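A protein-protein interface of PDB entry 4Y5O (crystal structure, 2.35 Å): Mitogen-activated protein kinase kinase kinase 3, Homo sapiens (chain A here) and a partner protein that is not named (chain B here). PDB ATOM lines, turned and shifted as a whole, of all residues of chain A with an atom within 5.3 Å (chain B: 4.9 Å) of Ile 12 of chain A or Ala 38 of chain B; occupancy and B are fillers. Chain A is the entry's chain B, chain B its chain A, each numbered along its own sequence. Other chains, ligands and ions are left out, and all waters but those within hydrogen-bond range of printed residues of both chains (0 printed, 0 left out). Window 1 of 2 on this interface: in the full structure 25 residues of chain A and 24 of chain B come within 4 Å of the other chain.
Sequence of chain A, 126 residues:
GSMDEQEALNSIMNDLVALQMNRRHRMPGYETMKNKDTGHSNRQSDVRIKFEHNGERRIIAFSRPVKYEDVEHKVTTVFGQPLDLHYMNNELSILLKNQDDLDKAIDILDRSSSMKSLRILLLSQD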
ATOM      1  N   ALA A   8      23.597  13.582   3.423  1.00  0.00           N
ATOM      2  CA  ALA A   8      23.715  14.960   3.920  1.00  0.00           C
ATOM      3  C   ALA A   8      22.771  15.898   3.174  1.00  0.00           C
ATOM      4  O   ALA A   8      22.014  16.642   3.789  1.00  0.00           O
ATOM      5  CB  ALA A   8      25.131  15.462   3.802  1.00  0.00           C
ATOM      6  N   LEU A   9      22.835  15.878   1.848  1.00  0.00           N
ATOM      7  CA  LEU A   9      22.010  16.778   1.035  1.00  0.00           C
ATOM      8  C   LEU A   9      20.518  16.606   1.304  1.00  0.00           C
ATOM      9  O   LEU A   9      19.773  17.577   1.265  1.00  0.00           O
ATOM     10  CB  LEU A   9      22.305  16.617  -0.456  1.00  0.00           C
ATOM     11  CG  LEU A   9      23.530  17.348  -0.993  1.00  0.00           C
ATOM     12  CD1 LEU A   9      23.712  17.077  -2.482  1.00  0.00           C
ATOM     13  CD2 LEU A   9      23.407  18.835  -0.729  1.00  0.00           C
ATOM     14  N   ASN A  10      20.098  15.374   1.588  1.00  0.00           N
ATOM     15  CA  ASN A  10      18.721  15.099   1.998  1.00  0.00           C
ATOM     16  C   ASN A  10      18.386  15.734   3.348  1.00  0.00           C
ATOM     17  O   ASN A  10      17.292  16.272   3.540  1.00  0.00           O
ATOM     18  CB  ASN A  10      18.479  13.587   2.071  1.00  0.00           C
ATOM     19  CG  ASN A  10      18.266  12.963   0.709  1.00  0.00           C
ATOM     20  OD1 ASN A  10      18.574  13.570  -0.310  1.00  0.00           O
ATOM     21  ND2 ASN A  10      17.726  11.746   0.686  1.00  0.00           N
ATOM     22  N   SER A  11      19.335  15.648   4.281  1.00  0.00           N
ATOM     23  CA  SER A  11      19.205  16.277   5.592  1.00  0.00           C
ATOM     24  C   SER A  11      19.059  17.787   5.441  1.00  0.00           C
ATOM     25  O   SER A  11      18.152  18.394   6.009  1.00  0.00           O
ATOM     26  CB  SER A  11      20.420  15.945   6.471  1.00  0.00           C
ATOM     27  OG  SER A  11      20.619  16.914   7.494  1.00  0.00           O
ATOM     28  N   ILE A  12      19.951  18.384   4.658  1.00  0.00           N
ATOM     29  CA  ILE A  12      19.921  19.828   4.433  1.00  0.00           C
ATOM     30  C   ILE A  12      18.584  20.264   3.839  1.00  0.00           C
ATOM     31  O   ILE A  12      18.063  21.333   4.160  1.00  0.00           O
ATOM     32  CB  ILE A  12      21.060  20.267   3.500  1.00  0.00           C
ATOM     33  CG1 ILE A  12      22.416  19.898   4.101  1.00  0.00           C
ATOM     34  CG2 ILE A  12      20.980  21.756   3.234  1.00  0.00           C
ATOM     35  CD1 ILE A  12      23.598  20.325   3.283  1.00  0.00           C
ATOM     36  N   MET A  13      18.025  19.417   2.984  1.00  0.00           N
ATOM     37  CA  MET A  13      16.791  19.751   2.301  1.00  0.00           C
ATOM     38  C   MET A  13      15.626  19.745   3.284  1.00  0.00           C
ATOM     39  O   MET A  13      14.832  20.683   3.316  1.00  0.00           O
ATOM     40  CB  MET A  13      16.528  18.783   1.147  1.00  0.00           C
ATOM     41  CG  MET A  13      15.244  19.086   0.393  1.00  0.00           C
ATOM     42  SD  MET A  13      14.810  17.784  -0.767  1.00  0.00           S
ATOM     43  CE  MET A  13      13.514  18.598  -1.697  1.00  0.00           C
ATOM     44  N   ASN A  14      15.539  18.695   4.093  1.00  0.00           N
ATOM     45  CA  ASN A  14      14.459  18.583   5.066  1.00  0.00           C
ATOM     46  C   ASN A  14      14.541  19.651   6.155  1.00  0.00           C
ATOM     47  O   ASN A  14      13.526  20.043   6.736  1.00  0.00           O
ATOM     48  CB  ASN A  14      14.445  17.187   5.684  1.00  0.00           C
ATOM     49  CG  ASN A  14      14.260  16.099   4.649  1.00  0.00           C
ATOM     50  OD1 ASN A  14      13.921  16.379   3.506  1.00  0.00           O
ATOM     51  ND2 ASN A  14      14.478  14.848   5.048  1.00  0.00           N
ATOM     52  N   ASP A  15      15.755  20.111   6.431  1.00  0.00           N
ATOM     53  CA  ASP A  15      15.961  21.160   7.425  1.00  0.00           C
ATOM     54  C   ASP A  15      15.479  22.512   6.886  1.00  0.00           C
ATOM     55  O   ASP A  15      14.761  23.237   7.570  1.00  0.00           O
ATOM     56  CB  ASP A  15      17.439  21.244   7.847  1.00  0.00           C
ATOM     57  CG  ASP A  15      17.845  20.145   8.830  1.00  0.00           C
ATOM     58  OD1 ASP A  15      16.944  19.511   9.423  1.00  0.00           O
ATOM     59  OD2 ASP A  15      19.071  19.928   9.010  1.00  0.00           O
ATOM     60  N   LEU A  16      15.871  22.839   5.656  1.00  0.00           N
ATOM     61  CA  LEU A  16      15.471  24.093   5.011  1.00  0.00           C
ATOM     62  C   LEU A  16      13.975  24.141   4.701  1.00  0.00           C
ATOM     63  O   LEU A  16      13.342  25.187   4.834  1.00  0.00           O
ATOM     64  CB  LEU A  16      16.286  24.328   3.736  1.00  0.00           C
ATOM     65  CG  LEU A  16      17.738  24.731   3.957  1.00  0.00           C
ATOM     66  CD1 LEU A  16      18.489  24.856   2.655  1.00  0.00           C
ATOM     67  CD2 LEU A  16      17.763  26.039   4.695  1.00  0.00           C
ATOM     68  N   VAL A  17      13.422  23.001   4.293  1.00  0.00           N
ATOM     69  CA  VAL A  17      11.998  22.884   3.986  1.00  0.00           C
ATOM     70  C   VAL A  17      11.202  23.097   5.270  1.00  0.00           C
ATOM     71  O   VAL A  17      10.023  23.441   5.245  1.00  0.00           O
ATOM     72  CB  VAL A  17      11.671  21.529   3.306  1.00  0.00           C
ATOM     73  CG1 VAL A  17      10.940  20.582   4.256  1.00  0.00           C
ATOM     74  CG2 VAL A  17      10.863  21.751   2.052  1.00  0.00           C
ATOM     75  N   ASN A  90      24.405  13.993   9.889  1.00  0.00           N
ATOM     76  CA  ASN A  90      23.210  14.525   9.235  1.00  0.00           C
ATOM     77  C   ASN A  90      22.094  14.830  10.246  1.00  0.00           C
ATOM     78  O   ASN A  90      22.336  15.531  11.218  1.00  0.00           O
ATOM     79  CB  ASN A  90      22.743  13.574   8.139  1.00  0.00           C
ATOM     80  CG  ASN A  90      23.858  13.216   7.166  1.00  0.00           C
ATOM     81  OD1 ASN A  90      24.791  13.987   6.955  1.00  0.00           O
ATOM     82  ND2 ASN A  90      23.758  12.039   6.565  1.00  0.00           N
ATOM     83  N   SER A  93      22.746  14.643  13.989  1.00  0.00           N
ATOM     84  CA  SER A  93      23.807  15.500  14.494  1.00  0.00           C
ATOM     85  C   SER A  93      23.317  16.320  15.688  1.00  0.00           C
ATOM     86  O   SER A  93      22.144  16.645  15.762  1.00  0.00           O
ATOM     87  CB  SER A  93      24.309  16.416  13.382  1.00  0.00           C
ATOM     88  OG  SER A  93      24.699  15.666  12.242  1.00  0.00           O
ATOM     89  N   MET B  22      20.030  23.974  -3.311  1.00  0.00           N
ATOM     90  CA  MET B  22      20.524  22.593  -3.235  1.00  0.00           C
ATOM     91  C   MET B  22      21.525  22.337  -4.348  1.00  0.00           C
ATOM     92  O   MET B  22      22.542  21.673  -4.153  1.00  0.00           O
ATOM     93  CB  MET B  22      19.380  21.584  -3.365  1.00  0.00           C
ATOM     94  CG  MET B  22      18.446  21.491  -2.167  1.00  0.00           C
ATOM     95  SD  MET B  22      19.265  21.002  -0.641  1.00  0.00           S
ATOM     96  CE  MET B  22      19.500  22.604   0.116  1.00  0.00           C
ATOM     97  N   LEU B  25      24.897  23.987  -3.531  1.00  0.00           N
ATOM     98  CA  LEU B  25      25.616  23.158  -2.563  1.00  0.00           C
ATOM     99  C   LEU B  25      26.237  21.918  -3.213  1.00  0.00           C
ATOM    100  O   LEU B  25      27.421  21.643  -3.028  1.00  0.00           O
ATOM    101  CB  LEU B  25      24.686  22.713  -1.439  1.00  0.00           C
ATOM    102  CG  LEU B  25      24.062  23.777  -0.558  1.00  0.00           C
ATOM    103  CD1 LEU B  25      23.246  23.102   0.516  1.00  0.00           C
ATOM    104  CD2 LEU B  25      25.143  24.651   0.040  1.00  0.00           C
ATOM    105  N   ILE B  34      29.857  19.408   2.877  1.00  0.00           N
ATOM    106  CA  ILE B  34      28.405  19.205   2.890  1.00  0.00           C
ATOM    107  C   ILE B  34      27.912  18.516   4.183  1.00  0.00           C
ATOM    108  O   ILE B  34      26.925  18.960   4.774  1.00  0.00           O
ATOM    109  CB  ILE B  34      27.919  18.415   1.658  1.00  0.00           C
ATOM    110  CG1 ILE B  34      28.293  19.147   0.371  1.00  0.00           C
ATOM    111  CG2 ILE B  34      26.416  18.224   1.703  1.00  0.00           C
ATOM    112  CD1 ILE B  34      27.840  18.450  -0.907  1.00  0.00           C
ATOM    113  N   GLN B  35      28.586  17.437   4.603  1.00  0.00           N
ATOM    114  CA  GLN B  35      28.229  16.721   5.833  1.00  0.00           C
ATOM    115  C   GLN B  35      28.403  17.643   7.027  1.00  0.00           C
ATOM    116  O   GLN B  35      27.515  17.734   7.878  1.00  0.00           O
ATOM    117  CB  GLN B  35      29.078  15.458   6.019  1.00  0.00           C
ATOM    118  CG  GLN B  35      29.153  14.544   4.782  1.00  0.00           C
ATOM    119  CD  GLN B  35      29.900  13.239   5.032  1.00  0.00           C
ATOM    120  OE1 GLN B  35      29.679  12.564   6.032  1.00  0.00           O
ATOM    121  NE2 GLN B  35      30.780  12.877   4.110  1.00  0.00           N
ATOM    122  N   GLN B  36      29.533  18.347   7.064  1.00  0.00           N
ATOM    123  CA  GLN B  36      29.787  19.334   8.110  1.00  0.00           C
ATOM    124  C   GLN B  36      28.679  20.385   8.164  1.00  0.00           C
ATOM    125  O   GLN B  36      28.090  20.609   9.218  1.00  0.00           O
ATOM    126  CB  GLN B  36      31.132  20.017   7.893  1.00  0.00           C
ATOM    127  CG  GLN B  36      32.320  19.092   8.017  1.00  0.00           C
ATOM    128  CD  GLN B  36      33.621  19.843   8.014  1.00  0.00           C
ATOM    129  OE1 GLN B  36      33.665  21.027   7.682  1.00  0.00           O
ATOM    130  NE2 GLN B  36      34.693  19.163   8.396  1.00  0.00           N
ATOM    131  N   PHE B  37      28.393  21.006   7.022  1.00  0.00           N
ATOM    132  CA  PHE B  37      27.320  21.994   6.931  1.00  0.00           C
ATOM    133  C   PHE B  37      25.960  21.426   7.329  1.00  0.00           C
ATOM    134  O   PHE B  37      25.226  22.063   8.074  1.00  0.00           O
ATOM    135  CB  PHE B  37      27.251  22.588   5.526  1.00  0.00           C
ATOM    136  CG  PHE B  37      26.129  23.559   5.340  1.00  0.00           C
ATOM    137  CD1 PHE B  37      26.098  24.754   6.043  1.00  0.00           C
ATOM    138  CD2 PHE B  37      25.101  23.281   4.456  1.00  0.00           C
ATOM    139  CE1 PHE B  37      25.059  25.647   5.866  1.00  0.00           C
ATOM    140  CE2 PHE B  37      24.057  24.170   4.275  1.00  0.00           C
ATOM    141  CZ  PHE B  37      24.036  25.352   4.977  1.00  0.00           C
ATOM    142  N   ALA B  38      25.635  20.226   6.855  1.00  0.00           N
ATOM    143  CA  ALA B  38      24.358  19.590   7.205  1.00  0.00           C
ATOM    144  C   ALA B  38      24.204  19.469   8.713  1.00  0.00           C
ATOM    145  O   ALA B  38      23.141  19.757   9.261  1.00  0.00           O
ATOM    146  CB  ALA B  38      24.232  18.220   6.549  1.00  0.00           C
ATOM    147  N   ALA B  39      25.287  19.054   9.365  1.00  0.00           N
ATOM    148  CA  ALA B  39      25.335  18.930  10.816  1.00  0.00           C
ATOM    149  C   ALA B  39      25.054  20.253  11.522  1.00  0.00           C
ATOM    150  O   ALA B  39      24.197  20.307  12.392  1.00  0.00           O
ATOM    151  CB  ALA B  39      26.674  18.364  11.255  1.00  0.00           C
ATOM    152  N   LEU B  40      25.776  21.313  11.166  1.00  0.00           N
ATOM    153  CA  LEU B  40      25.524  22.611  11.790  1.00  0.00           C
ATOM    154  C   LEU B  40      24.100  23.055  11.512  1.00  0.00           C
ATOM    155  O   LEU B  40      23.398  23.512  12.408  1.00  0.00           O
ATOM    156  CB  LEU B  40      26.495  23.674  11.284  1.00  0.00           C
ATOM    157  CG  LEU B  40      27.957  23.500  11.667  1.00  0.00           C
ATOM    158  CD1 LEU B  40      28.767  24.737  11.319  1.00  0.00           C
ATOM    159  CD2 LEU B  40      28.076  23.184  13.144  1.00  0.00           C
ATOM    160  N   LEU B  41      23.673  22.911  10.263  1.00  0.00           N
ATOM    161  CA  LEU B  41      22.331  23.323   9.882  1.00  0.00           C
ATOM    162  C   LEU B  41      21.297  22.563  10.680  1.00  0.00           C
ATOM    163  O   LEU B  41      20.239  23.087  10.978  1.00  0.00           O
ATOM    164  CB  LEU B  41      22.085  23.084   8.398  1.00  0.00           C
ATOM    165  CG  LEU B  41      20.795  23.722   7.888  1.00  0.00           C
ATOM    166  CD1 LEU B  41      20.984  25.215   7.753  1.00  0.00           C
ATOM    167  CD2 LEU B  41      20.365  23.126   6.573  1.00  0.00           C
ATOM    168  N   HIS B  42      21.587  21.319  11.038  1.00  0.00           N
ATOM    169  CA  HIS B  42      20.595  20.581  11.803  1.00  0.00           C
ATOM    170  C   HIS B  42      20.479  21.140  13.232  1.00  0.00           C
ATOM    171  O   HIS B  42      19.369  21.255  13.769  1.00  0.00           O
ATOM    172  CB  HIS B  42      20.889  19.088  11.795  1.00  0.00           C
ATOM    173  CG  HIS B  42      19.723  18.248  12.201  1.00  0.00           C
ATOM    174  ND1 HIS B  42      18.464  18.419  11.669  1.00  0.00           N
ATOM    175  CD2 HIS B  42      19.622  17.229  13.086  1.00  0.00           C
ATOM    176  CE1 HIS B  42      17.637  17.543  12.209  1.00  0.00           C
ATOM    177  NE2 HIS B  42      18.316  16.807  13.070  1.00  0.00           N
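A ring nitrogen (ND1) of His 42 of chain B lies within hydrogen-bond range of the side-chain carboxylate of Asp 15 of chain A (2.9 Å).
O of Asn 90 of chain A lies within hydrogen-bond range of OG of Ser 93 of chain A (2.6 Å).
Among the printed residues, pairs that only touch across the chains: Ala 8 of chain A with Ile 34 of chain B, Ala 8 of chain A with Gln 35 of chain B, Ala 8 of chain A with Ala 38 of chain B, Leu 9 of chain A with Met 22 of chain B, Leu 9 of chain A with Ile 34 of chain B, Ser 11 of chain A with Ala 38 of chain B, Ile 12 of chain A with Met 22 of chain B, Ile 12 of chain A with Leu 25 of chain B, Ile 12 of chain A with Ile 34 of chain B, Ile 12 of chain A with Phe 37 of chain B, Ile 12 of chain A with Ala 38 of chain B, Ile 12 of chain A with Leu 41 of chain B, Met 13 of chain A with Met 22 of chain B, Asp 15 of chain A with Leu 41 of chain B, Leu 16 of chain A with Met 22 of chain B, Asn 90 of chain A with His 42 of chain B, Ser 93 of chain A with Ala 39 of chain B and Ser 93 of chain A with His 42 of chain B.
Printed residues of chain B within 4 Å of Leu 9 of chain A: Met 22 and Ile 34.
Of the printed residues of chain B, Ile 12 of chain A touches Met 22, Leu 25, Ile 34, Phe 37, Ala 38 and Leu 41.
Printed residues of chain B within 4 Å of Met 13 of chain A: Met 22 (3.95 Å).
Printed residues of chain B within 4 Å of Ser 93 of chain A: Ala 39 (3.5 Å) and His 42 (3.7 Å).
Printed residues of chain A within 4 Å of Leu 25 of chain B: Ile 12 (3.8 Å).
Of the printed residues of chain A, Gln 35 of chain B touches Ala 8 (3.9 Å).
Gln 36 of chain B touches none of the printed residues of chain A.
Ala 38 of chain B touches three residues of chain A.
The nearest residue of chain A that does not touch Ala 38 of chain B is Asp 15 of chain A (4.1 Å).
Printed residues of chain A that touch a printed residue of chain B: Ala 8, Leu 9, Ser 11, Ile 12, Met 13, Asp 15, Leu 16, Asn 90 and Ser 93.
Hydrophobic or aromatic side chains of chain A within 4 Å of the printed part of chain B: Ala 8, Leu 9, Ile 12, Met 13 and Leu 16.
Of the 11 printed residues of chain B, 9 touch a printed residue of chain A.
Among the printed residues, 19 pairs touch across the chains.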
